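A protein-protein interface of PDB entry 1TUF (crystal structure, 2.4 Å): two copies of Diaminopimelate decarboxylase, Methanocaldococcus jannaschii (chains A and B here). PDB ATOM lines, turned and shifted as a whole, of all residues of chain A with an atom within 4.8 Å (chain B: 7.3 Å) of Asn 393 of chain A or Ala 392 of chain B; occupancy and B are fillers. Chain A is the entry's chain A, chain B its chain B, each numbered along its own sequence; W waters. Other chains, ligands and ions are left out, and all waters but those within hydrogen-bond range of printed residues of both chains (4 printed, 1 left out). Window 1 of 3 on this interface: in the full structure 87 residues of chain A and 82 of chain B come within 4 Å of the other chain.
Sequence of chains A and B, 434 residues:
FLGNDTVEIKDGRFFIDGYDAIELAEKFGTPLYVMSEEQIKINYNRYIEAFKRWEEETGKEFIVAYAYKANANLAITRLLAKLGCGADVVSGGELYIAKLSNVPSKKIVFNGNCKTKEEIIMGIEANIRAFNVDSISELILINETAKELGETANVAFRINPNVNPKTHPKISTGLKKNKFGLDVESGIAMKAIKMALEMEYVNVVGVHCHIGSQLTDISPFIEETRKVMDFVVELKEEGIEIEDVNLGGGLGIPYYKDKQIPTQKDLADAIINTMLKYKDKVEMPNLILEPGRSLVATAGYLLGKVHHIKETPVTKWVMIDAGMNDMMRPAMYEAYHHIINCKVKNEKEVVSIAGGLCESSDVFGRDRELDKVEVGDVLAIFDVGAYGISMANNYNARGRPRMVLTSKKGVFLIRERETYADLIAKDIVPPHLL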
ATOM      1  N   ASN A 325      17.348  35.428  25.921  1.00  0.00           N
ATOM      2  CA  ASN A 325      18.191  34.426  25.266  1.00  0.00           C
ATOM      3  C   ASN A 325      19.022  33.721  26.329  1.00  0.00           C
ATOM      4  O   ASN A 325      19.321  32.536  26.208  1.00  0.00           O
ATOM      5  CB  ASN A 325      19.130  35.059  24.236  1.00  0.00           C
ATOM      6  CG  ASN A 325      20.141  35.982  24.873  1.00  0.00           C
ATOM      7  OD1 ASN A 325      19.785  37.052  25.373  1.00  0.00           O
ATOM      8  ND2 ASN A 325      21.407  35.568  24.881  1.00  0.00           N
ATOM      9  N   MET A 328      15.294  31.785  29.217  1.00  0.00           N
ATOM     10  CA  MET A 328      14.004  31.801  28.537  1.00  0.00           C
ATOM     11  C   MET A 328      12.718  31.628  29.336  1.00  0.00           C
ATOM     12  O   MET A 328      11.645  31.991  28.855  1.00  0.00           O
ATOM     13  CB  MET A 328      14.021  30.741  27.433  1.00  0.00           C
ATOM     14  CG  MET A 328      14.979  31.037  26.285  1.00  0.00           C
ATOM     15  SD  MET A 328      14.371  32.348  25.195  1.00  0.00           S
ATOM     16  CE  MET A 328      13.176  31.436  24.194  1.00  0.00           C
ATOM     17  N   MET A 391      18.329  26.063  28.060  1.00  0.00           N
ATOM     18  CA  MET A 391      17.412  26.515  27.021  1.00  0.00           C
ATOM     19  C   MET A 391      17.865  27.849  26.437  1.00  0.00           C
ATOM     20  O   MET A 391      17.141  28.471  25.673  1.00  0.00           O
ATOM     21  CB  MET A 391      15.992  26.653  27.574  1.00  0.00           C
ATOM     22  CG  MET A 391      15.449  25.371  28.176  1.00  0.00           C
ATOM     23  SD  MET A 391      13.647  25.376  28.277  1.00  0.00           S
ATOM     24  CE  MET A 391      13.313  26.858  29.329  1.00  0.00           C
ATOM     25  N   ALA A 392      19.068  28.276  26.804  1.00  0.00           N
ATOM     26  CA  ALA A 392      19.621  29.536  26.331  1.00  0.00           C
ATOM     27  C   ALA A 392      19.991  29.451  24.848  1.00  0.00           C
ATOM     28  O   ALA A 392      20.309  28.369  24.331  1.00  0.00           O
ATOM     29  CB  ALA A 392      20.848  29.902  27.162  1.00  0.00           C
ATOM     30  N   ASN A 393      19.979  30.601  24.175  1.00  0.00           N
ATOM     31  CA  ASN A 393      20.285  30.651  22.751  1.00  0.00           C
ATOM     32  C   ASN A 393      20.936  31.976  22.339  1.00  0.00           C
ATOM     33  O   ASN A 393      21.307  32.788  23.189  1.00  0.00           O
ATOM     34  CB  ASN A 393      18.998  30.465  21.968  1.00  0.00           C
ATOM     35  CG  ASN A 393      17.938  31.426  22.414  1.00  0.00           C
ATOM     36  OD1 ASN A 393      16.941  31.021  23.006  1.00  0.00           O
ATOM     37  ND2 ASN A 393      18.162  32.722  22.175  1.00  0.00           N
ATOM     38  N   ASN A 394      21.039  32.190  21.023  1.00  0.00           N
ATOM     39  CA  ASN A 394      21.653  33.393  20.468  1.00  0.00           C
ATOM     40  C   ASN A 394      20.668  34.334  19.791  1.00  0.00           C
ATOM     41  O   ASN A 394      21.046  35.133  18.928  1.00  0.00           O
ATOM     42  CB  ASN A 394      22.746  33.012  19.468  1.00  0.00           C
ATOM     43  CG  ASN A 394      23.933  32.331  20.132  1.00  0.00           C
ATOM     44  OD1 ASN A 394      24.427  32.785  21.173  1.00  0.00           O
ATOM     45  ND2 ASN A 394      24.410  31.252  19.525  1.00  0.00           N
ATOM     46  N   TYR A 395      19.406  34.248  20.188  1.00  0.00           N
ATOM     47  CA  TYR A 395      18.384  35.105  19.614  1.00  0.00           C
ATOM     48  C   TYR A 395      18.858  36.551  19.699  1.00  0.00           C
ATOM     49  O   TYR A 395      19.461  36.965  20.703  1.00  0.00           O
ATOM     50  CB  TYR A 395      17.070  34.910  20.361  1.00  0.00           C
ATOM     51  CG  TYR A 395      15.914  35.646  19.746  1.00  0.00           C
ATOM     52  CD1 TYR A 395      15.776  35.738  18.348  1.00  0.00           C
ATOM     53  CD2 TYR A 395      14.934  36.231  20.552  1.00  0.00           C
ATOM     54  CE1 TYR A 395      14.688  36.393  17.773  1.00  0.00           C
ATOM     55  CE2 TYR A 395      13.845  36.886  19.993  1.00  0.00           C
ATOM     56  CZ  TYR A 395      13.723  36.962  18.606  1.00  0.00           C
ATOM     57  OH  TYR A 395      12.615  37.571  18.077  1.00  0.00           O
ATOM     58  N   ARG A 398      22.978  37.290  20.158  1.00  0.00           N
ATOM     59  CA  ARG A 398      23.587  37.513  21.468  1.00  0.00           C
ATOM     60  C   ARG A 398      24.232  36.207  21.930  1.00  0.00           C
ATOM     61  O   ARG A 398      23.625  35.143  21.831  1.00  0.00           O
ATOM     62  CB  ARG A 398      22.529  37.945  22.484  1.00  0.00           C
ATOM     63  CG  ARG A 398      22.200  39.434  22.492  1.00  0.00           C
ATOM     64  CD  ARG A 398      21.205  39.727  23.620  1.00  0.00           C
ATOM     65  NE  ARG A 398      21.225  41.119  24.087  1.00  0.00           N
ATOM     66  CZ  ARG A 398      20.787  42.165  23.388  1.00  0.00           C
ATOM     67  NH1 ARG A 398      20.284  41.996  22.169  1.00  0.00           N
ATOM     68  NH2 ARG A 398      20.837  43.383  23.913  1.00  0.00           N
ATOM     69  N   GLY A 399      25.463  36.280  22.420  1.00  0.00           N
ATOM     70  CA  GLY A 399      26.128  35.070  22.866  1.00  0.00           C
ATOM     71  C   GLY A 399      25.570  34.579  24.188  1.00  0.00           C
ATOM     72  O   GLY A 399      24.974  35.349  24.935  1.00  0.00           O
ATOM     73  N   ARG A 400      25.733  33.292  24.476  1.00  0.00           N
ATOM     74  CA  ARG A 400      25.249  32.765  25.739  1.00  0.00           C
ATOM     75  C   ARG A 400      26.170  33.240  26.852  1.00  0.00           C
ATOM     76  O   ARG A 400      27.390  33.343  26.674  1.00  0.00           O
ATOM     77  CB  ARG A 400      25.180  31.246  25.702  1.00  0.00           C
ATOM     78  CG  ARG A 400      23.970  30.741  24.944  1.00  0.00           C
ATOM     79  CD  ARG A 400      24.405  29.978  23.727  1.00  0.00           C
ATOM     80  NE  ARG A 400      24.238  28.547  23.898  1.00  0.00           N
ATOM     81  CZ  ARG A 400      24.848  27.639  23.147  1.00  0.00           C
ATOM     82  NH1 ARG A 400      25.670  28.020  22.184  1.00  0.00           N
ATOM     83  NH2 ARG A 400      24.626  26.349  23.349  1.00  0.00           N
ATOM     84  N   TYR B  33      17.816  22.364   7.478  1.00  0.00           N
ATOM     85  CA  TYR B  33      17.191  23.623   7.099  1.00  0.00           C
ATOM     86  C   TYR B  33      17.587  23.824   5.628  1.00  0.00           C
ATOM     87  O   TYR B  33      18.753  23.649   5.269  1.00  0.00           O
ATOM     88  CB  TYR B  33      17.764  24.778   7.929  1.00  0.00           C
ATOM     89  CG  TYR B  33      16.921  25.206   9.102  1.00  0.00           C
ATOM     90  CD1 TYR B  33      15.773  25.977   8.914  1.00  0.00           C
ATOM     91  CD2 TYR B  33      17.254  24.821  10.397  1.00  0.00           C
ATOM     92  CE1 TYR B  33      14.973  26.357   9.984  1.00  0.00           C
ATOM     93  CE2 TYR B  33      16.464  25.191  11.480  1.00  0.00           C
ATOM     94  CZ  TYR B  33      15.321  25.960  11.270  1.00  0.00           C
ATOM     95  OH  TYR B  33      14.538  26.316  12.353  1.00  0.00           O
ATOM     96  N   MET B 324      12.005  20.666  18.526  1.00  0.00           N
ATOM     97  CA  MET B 324      11.729  22.059  18.843  1.00  0.00           C
ATOM     98  C   MET B 324      12.989  22.896  19.034  1.00  0.00           C
ATOM     99  O   MET B 324      12.961  24.116  18.850  1.00  0.00           O
ATOM    100  CB  MET B 324      10.864  22.148  20.099  1.00  0.00           C
ATOM    101  CG  MET B 324      11.555  21.613  21.336  1.00  0.00           C
ATOM    102  SD  MET B 324      10.562  21.776  22.819  1.00  0.00           S
ATOM    103  CE  MET B 324      10.891  23.474  23.294  1.00  0.00           C
ATOM    104  N   ASN B 325      14.091  22.255  19.417  1.00  0.00           N
ATOM    105  CA  ASN B 325      15.340  22.988  19.609  1.00  0.00           C
ATOM    106  C   ASN B 325      15.839  23.466  18.245  1.00  0.00           C
ATOM    107  O   ASN B 325      16.662  24.379  18.163  1.00  0.00           O
ATOM    108  CB  ASN B 325      16.408  22.101  20.264  1.00  0.00           C
ATOM    109  CG  ASN B 325      16.945  21.051  19.326  1.00  0.00           C
ATOM    110  OD1 ASN B 325      16.194  20.217  18.823  1.00  0.00           O
ATOM    111  ND2 ASN B 325      18.256  21.087  19.076  1.00  0.00           N
ATOM    112  N   ASP B 326      15.339  22.844  17.177  1.00  0.00           N
ATOM    113  CA  ASP B 326      15.737  23.223  15.822  1.00  0.00           C
ATOM    114  C   ASP B 326      14.852  24.355  15.299  1.00  0.00           C
ATOM    115  O   ASP B 326      15.308  25.254  14.591  1.00  0.00           O
ATOM    116  CB  ASP B 326      15.629  22.034  14.853  1.00  0.00           C
ATOM    117  CG  ASP B 326      16.528  20.869  15.234  1.00  0.00           C
ATOM    118  OD1 ASP B 326      17.679  21.112  15.649  1.00  0.00           O
ATOM    119  OD2 ASP B 326      16.086  19.710  15.110  1.00  0.00           O
ATOM    120  N   MET B 327      13.580  24.301  15.663  1.00  0.00           N
ATOM    121  CA  MET B 327      12.610  25.291  15.228  1.00  0.00           C
ATOM    122  C   MET B 327      11.563  25.386  16.353  1.00  0.00           C
ATOM    123  O   MET B 327      10.647  24.568  16.446  1.00  0.00           O
ATOM    124  CB  MET B 327      12.003  24.816  13.907  1.00  0.00           C
ATOM    125  CG  MET B 327      11.524  25.920  13.019  1.00  0.00           C
ATOM    126  SD  MET B 327      10.092  26.652  13.708  1.00  0.00           S
ATOM    127  CE  MET B 327       8.851  25.638  12.977  1.00  0.00           C
ATOM    128  N   MET B 328      11.733  26.393  17.207  1.00  0.00           N
ATOM    129  CA  MET B 328      10.896  26.625  18.389  1.00  0.00           C
ATOM    130  C   MET B 328       9.500  27.200  18.223  1.00  0.00           C
ATOM    131  O   MET B 328       8.749  27.281  19.195  1.00  0.00           O
ATOM    132  CB  MET B 328      11.645  27.543  19.354  1.00  0.00           C
ATOM    133  CG  MET B 328      12.862  26.928  20.023  1.00  0.00           C
ATOM    134  SD  MET B 328      12.380  25.891  21.413  1.00  0.00           S
ATOM    135  CE  MET B 328      11.838  27.149  22.547  1.00  0.00           C
ATOM    136  N   MET B 332       6.654  26.843  21.082  1.00  0.00           N
ATOM    137  CA  MET B 332       6.669  28.069  21.856  1.00  0.00           C
ATOM    138  C   MET B 332       5.435  28.944  21.699  1.00  0.00           C
ATOM    139  O   MET B 332       4.973  29.555  22.660  1.00  0.00           O
ATOM    140  CB  MET B 332       7.922  28.863  21.504  1.00  0.00           C
ATOM    141  CG  MET B 332       8.270  29.949  22.488  1.00  0.00           C
ATOM    142  SD  MET B 332       9.909  30.656  22.142  1.00  0.00           S
ATOM    143  CE  MET B 332       9.674  32.373  22.683  1.00  0.00           C
ATOM    144  N   TYR B 387      12.797  33.389  12.303  1.00  0.00           N
ATOM    145  CA  TYR B 387      12.606  32.999  13.693  1.00  0.00           C
ATOM    146  C   TYR B 387      12.673  31.489  13.803  1.00  0.00           C
ATOM    147  O   TYR B 387      11.937  30.873  14.573  1.00  0.00           O
ATOM    148  CB  TYR B 387      11.262  33.518  14.204  1.00  0.00           C
ATOM    149  CG  TYR B 387      11.155  35.009  14.035  1.00  0.00           C
ATOM    150  CD1 TYR B 387      12.029  35.866  14.721  1.00  0.00           C
ATOM    151  CD2 TYR B 387      10.264  35.566  13.109  1.00  0.00           C
ATOM    152  CE1 TYR B 387      12.028  37.238  14.484  1.00  0.00           C
ATOM    153  CE2 TYR B 387      10.255  36.945  12.863  1.00  0.00           C
ATOM    154  CZ  TYR B 387      11.141  37.769  13.552  1.00  0.00           C
ATOM    155  OH  TYR B 387      11.158  39.118  13.315  1.00  0.00           O
ATOM    156  N   GLY B 388      13.557  30.906  13.004  1.00  0.00           N
ATOM    157  CA  GLY B 388      13.748  29.473  13.018  1.00  0.00           C
ATOM    158  C   GLY B 388      15.130  29.209  13.589  1.00  0.00           C
ATOM    159  O   GLY B 388      15.297  29.022  14.797  1.00  0.00           O
ATOM    160  N   ILE B 389      16.139  29.224  12.730  1.00  0.00           N
ATOM    161  CA  ILE B 389      17.479  28.990  13.207  1.00  0.00           C
ATOM    162  C   ILE B 389      17.851  30.097  14.182  1.00  0.00           C
ATOM    163  O   ILE B 389      18.592  29.867  15.134  1.00  0.00           O
ATOM    164  CB  ILE B 389      18.514  28.955  12.048  1.00  0.00           C
ATOM    165  CG1 ILE B 389      19.882  28.549  12.589  1.00  0.00           C
ATOM    166  CG2 ILE B 389      18.617  30.304  11.371  1.00  0.00           C
ATOM    167  CD1 ILE B 389      19.957  27.095  12.997  1.00  0.00           C
ATOM    168  N   SER B 390      17.319  31.294  13.979  1.00  0.00           N
ATOM    169  CA  SER B 390      17.655  32.384  14.879  1.00  0.00           C
ATOM    170  C   SER B 390      17.225  32.126  16.318  1.00  0.00           C
ATOM    171  O   SER B 390      17.800  32.697  17.247  1.00  0.00           O
ATOM    172  CB  SER B 390      17.054  33.712  14.387  1.00  0.00           C
ATOM    173  OG  SER B 390      15.675  33.807  14.677  1.00  0.00           O
ATOM    174  N   MET B 391      16.226  31.270  16.514  1.00  0.00           N
ATOM    175  CA  MET B 391      15.774  30.969  17.870  1.00  0.00           C
ATOM    176  C   MET B 391      16.123  29.537  18.304  1.00  0.00           C
ATOM    177  O   MET B 391      15.765  29.115  19.402  1.00  0.00           O
ATOM    178  CB  MET B 391      14.261  31.227  18.015  1.00  0.00           C
ATOM    179  CG  MET B 391      13.865  32.694  17.836  1.00  0.00           C
ATOM    180  SD  MET B 391      12.175  33.144  18.371  1.00  0.00           S
ATOM    181  CE  MET B 391      11.145  32.102  17.303  1.00  0.00           C
ATOM    182  N   ALA B 392      16.841  28.807  17.451  1.00  0.00           N
ATOM    183  CA  ALA B 392      17.237  27.435  17.760  1.00  0.00           C
ATOM    184  C   ALA B 392      18.089  27.388  19.024  1.00  0.00           C
ATOM    185  O   ALA B 392      18.645  28.403  19.448  1.00  0.00           O
ATOM    186  CB  ALA B 392      18.005  26.839  16.606  1.00  0.00           C
ATOM    187  N   ASN B 393      18.191  26.211  19.629  1.00  0.00           N
ATOM    188  CA  ASN B 393      18.986  26.054  20.843  1.00  0.00           C
ATOM    189  C   ASN B 393      19.470  24.623  20.943  1.00  0.00           C
ATOM    190  O   ASN B 393      19.329  23.854  20.002  1.00  0.00           O
ATOM    191  CB  ASN B 393      18.152  26.385  22.074  1.00  0.00           C
ATOM    192  CG  ASN B 393      16.845  25.639  22.083  1.00  0.00           C
ATOM    193  OD1 ASN B 393      15.773  26.231  21.913  1.00  0.00           O
ATOM    194  ND2 ASN B 393      16.920  24.326  22.243  1.00  0.00           N
ATOM    195  N   ASN B 394      20.030  24.268  22.096  1.00  0.00           N
ATOM    196  CA  ASN B 394      20.539  22.927  22.310  1.00  0.00           C
ATOM    197  C   ASN B 394      19.771  22.166  23.383  1.00  0.00           C
ATOM    198  O   ASN B 394      20.306  21.231  23.982  1.00  0.00           O
ATOM    199  CB  ASN B 394      22.017  22.971  22.698  1.00  0.00           C
ATOM    200  CG  ASN B 394      22.901  23.424  21.564  1.00  0.00           C
ATOM    201  OD1 ASN B 394      22.829  22.897  20.457  1.00  0.00           O
ATOM    202  ND2 ASN B 394      23.752  24.393  21.834  1.00  0.00           N
ATOM    203  N   TYR B 395      18.524  22.561  23.629  1.00  0.00           N
ATOM    204  CA  TYR B 395      17.693  21.893  24.629  1.00  0.00           C
ATOM    205  C   TYR B 395      17.785  20.381  24.439  1.00  0.00           C
ATOM    206  O   TYR B 395      17.773  19.892  23.316  1.00  0.00           O
ATOM    207  CB  TYR B 395      16.247  22.357  24.494  1.00  0.00           C
ATOM    208  CG  TYR B 395      15.374  21.951  25.654  1.00  0.00           C
ATOM    209  CD1 TYR B 395      15.855  22.020  26.966  1.00  0.00           C
ATOM    210  CD2 TYR B 395      14.059  21.535  25.453  1.00  0.00           C
ATOM    211  CE1 TYR B 395      15.050  21.690  28.044  1.00  0.00           C
ATOM    212  CE2 TYR B 395      13.242  21.202  26.526  1.00  0.00           C
ATOM    213  CZ  TYR B 395      13.741  21.284  27.818  1.00  0.00           C
ATOM    214  OH  TYR B 395      12.923  20.993  28.883  1.00  0.00           O
ATOM    215  N   GLY B 399      22.651  19.503  19.284  1.00  0.00           N
ATOM    216  CA  GLY B 399      23.256  20.627  18.581  1.00  0.00           C
ATOM    217  C   GLY B 399      22.324  21.186  17.524  1.00  0.00           C
ATOM    218  O   GLY B 399      21.455  20.469  17.024  1.00  0.00           O
ATOM    219  N   ARG B 400      22.477  22.465  17.188  1.00  0.00           N
ATOM    220  CA  ARG B 400      21.619  23.043  16.157  1.00  0.00           C
ATOM    221  C   ARG B 400      21.906  22.355  14.841  1.00  0.00           C
ATOM    222  O   ARG B 400      23.034  21.935  14.577  1.00  0.00           O
ATOM    223  CB  ARG B 400      21.827  24.539  16.016  1.00  0.00           C
ATOM    224  CG  ARG B 400      21.449  25.301  17.244  1.00  0.00           C
ATOM    225  CD  ARG B 400      22.682  25.597  18.014  1.00  0.00           C
ATOM    226  NE  ARG B 400      22.793  27.020  18.254  1.00  0.00           N
ATOM    227  CZ  ARG B 400      23.928  27.645  18.535  1.00  0.00           C
ATOM    228  NH1 ARG B 400      25.077  26.985  18.611  1.00  0.00           N
ATOM    229  NH2 ARG B 400      23.904  28.943  18.749  1.00  0.00           N
ATOM    230  N   PRO B 401      20.886  22.252  13.986  1.00  0.00           N
ATOM    231  CA  PRO B 401      20.966  21.600  12.676  1.00  0.00           C
ATOM    232  C   PRO B 401      21.817  22.235  11.573  1.00  0.00           C
ATOM    233  O   PRO B 401      22.344  23.334  11.711  1.00  0.00           O
ATOM    234  CB  PRO B 401      19.507  21.497  12.273  1.00  0.00           C
ATOM    235  CG  PRO B 401      18.981  22.819  12.756  1.00  0.00           C
ATOM    236  CD  PRO B 401      19.612  22.981  14.126  1.00  0.00           C
ATOM    237  N   ARG B 415      25.513  26.401   6.968  1.00  0.00           N
ATOM    238  CA  ARG B 415      25.636  26.266   8.419  1.00  0.00           C
ATOM    239  C   ARG B 415      25.960  24.812   8.749  1.00  0.00           C
ATOM    240  O   ARG B 415      25.231  23.905   8.372  1.00  0.00           O
ATOM    241  CB  ARG B 415      24.352  26.689   9.129  1.00  0.00           C
ATOM    242  CG  ARG B 415      24.542  26.776  10.639  1.00  0.00           C
ATOM    243  CD  ARG B 415      23.258  26.563  11.440  1.00  0.00           C
ATOM    244  NE  ARG B 415      23.597  26.217  12.814  1.00  0.00           N
ATOM    245  CZ  ARG B 415      23.915  27.096  13.761  1.00  0.00           C
ATOM    246  NH1 ARG B 415      23.920  28.399  13.508  1.00  0.00           N
ATOM    247  NH2 ARG B 415      24.279  26.664  14.959  1.00  0.00           N
HETATM  248  O   HOH W   1      26.736  25.212  21.259  1.00  0.00           O
HETATM  249  O   HOH W   2      20.472  25.725  24.337  1.00  0.00           O
HETATM  250  O   HOH W   3      20.429  33.174  16.733  1.00  0.00           O
HETATM  251  O   HOH W   4      20.084  30.575  19.099  1.00  0.00           O
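Of chain B, only Ala 392 (3.3 Å) comes within 4 Å of Asn 393 of chain A.
Met 328 of chain B touches none of the printed residues of chain A.
Of the printed residues of chain A, Ser 390 of chain B touches Tyr 395.
Of chain A, only Asn 393 comes within 4 Å of Ala 392 of chain B.
Gly 399 of chain B touches none of the printed residues of chain A.
Of the printed residues of chain A, Arg 400 of chain B touches Asn 394 (2.5 Å) and Arg 400 (3.8 Å).
The nearest residue of chain B that does not touch Asn 393 of chain A is Asn 393 of chain B (4.2 Å).
The nearest residue of chain A that does not touch Ala 392 of chain B is Asn 394 of chain A (4.7 Å).
Met 391 of chain A touches Tyr 395 of chain B, and with the chains exchanged Tyr 395 of chain A touches Met 391 of chain B.
Ala 392 of chain A touches Asn 393 of chain B, and with the chains exchanged Asn 393 of chain A touches Ala 392 of chain B.
Asn 394 of chain A touches Arg 400 of chain B, and with the chains exchanged Arg 400 of chain A touches Asn 394 of chain B.
Arg 400 of chain A touches its own counterpart, Arg 400 of chain B.
Positions printed for both chains: 325, 328, 391, 392, 393, 394, 395, 399 and 400.
Of the 10 pairs that touch across the chains among the printed residues, 7 have their exchanged pair printed and touching as well.
O of Asn 325 of chain A lies within hydrogen-bond range of N of Asn 393 of chain A, 2.9 Å away.
N of Tyr 395 of chain A lies close to ND2 of Asn 393 of chain A, 2.8 Å away.
The backbone carbonyl oxygen (O) of Arg 398 of chain A lies close to the side-chain amide oxygen (OD1) of Asn 394 of chain A, at 2.6 Å.
The backbone carbonyl oxygen of Asn 325 of chain B is in hydrogen-bond range of the backbone NH of Asn 393 of chain B.
N of Tyr 395 of chain B lies close to ND2 of Asn 393 of chain B (2.8 Å).
OD1 of Asn 394 of chain B is in hydrogen-bond range of N of Arg 400 of chain B (3.3 Å).
Hydrophobic or aromatic side chains of chain B within 4 Å of the printed part of chain A: Met 332, Tyr 387, Met 391 and Tyr 395.
Printed residues of chain A that touch a printed residue of chain B: Met 328, Met 391, Ala 392, Asn 393, Asn 394, Tyr 395 and Arg 400.
NH2 of Arg 400 of chain B lies close to ND2 of Asn 394 of chain A (2.5 Å).
NH2 of Arg 400 of chain A lies close to ND2 of Asn 394 of chain B.
Water W4 bridges O of Ala 392 of chain B and N of Asn 394 of chain A.
Water W2 lies within hydrogen-bond range of the backbone carbonyl oxygen of Ala 392 of chain A (2.6 Å) and the backbone NH of Asn 394 of chain B (2.7 Å).
Water W3 lies within hydrogen-bond range of the backbone carbonyl oxygen (O) of Ser 390 of chain B (2.7 Å) and the backbone carbonyl oxygen (O) of Asn 394 of chain A (3.0 Å).
Water W1 bridges the guanidinium group of Arg 400 of chain A (3.1 Å) and the side-chain amide nitrogen of Asn 394 of chain B (3.1 Å).
Among the printed residues, merely in contact across the chains: Met 328 of chain A with Met 332 of chain B, Met 391 of chain A with Tyr 395 of chain B, Ala 392 of chain A with Asn 393 of chain B, Asn 393 of chain A with Ala 392 of chain B, Tyr 395 of chain A with Tyr 387 of chain B, Tyr 395 of chain A with Ser 390 of chain B, Tyr 395 of chain A with Met 391 of chain B and Arg 400 of chain A with Arg 400 of chain B.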
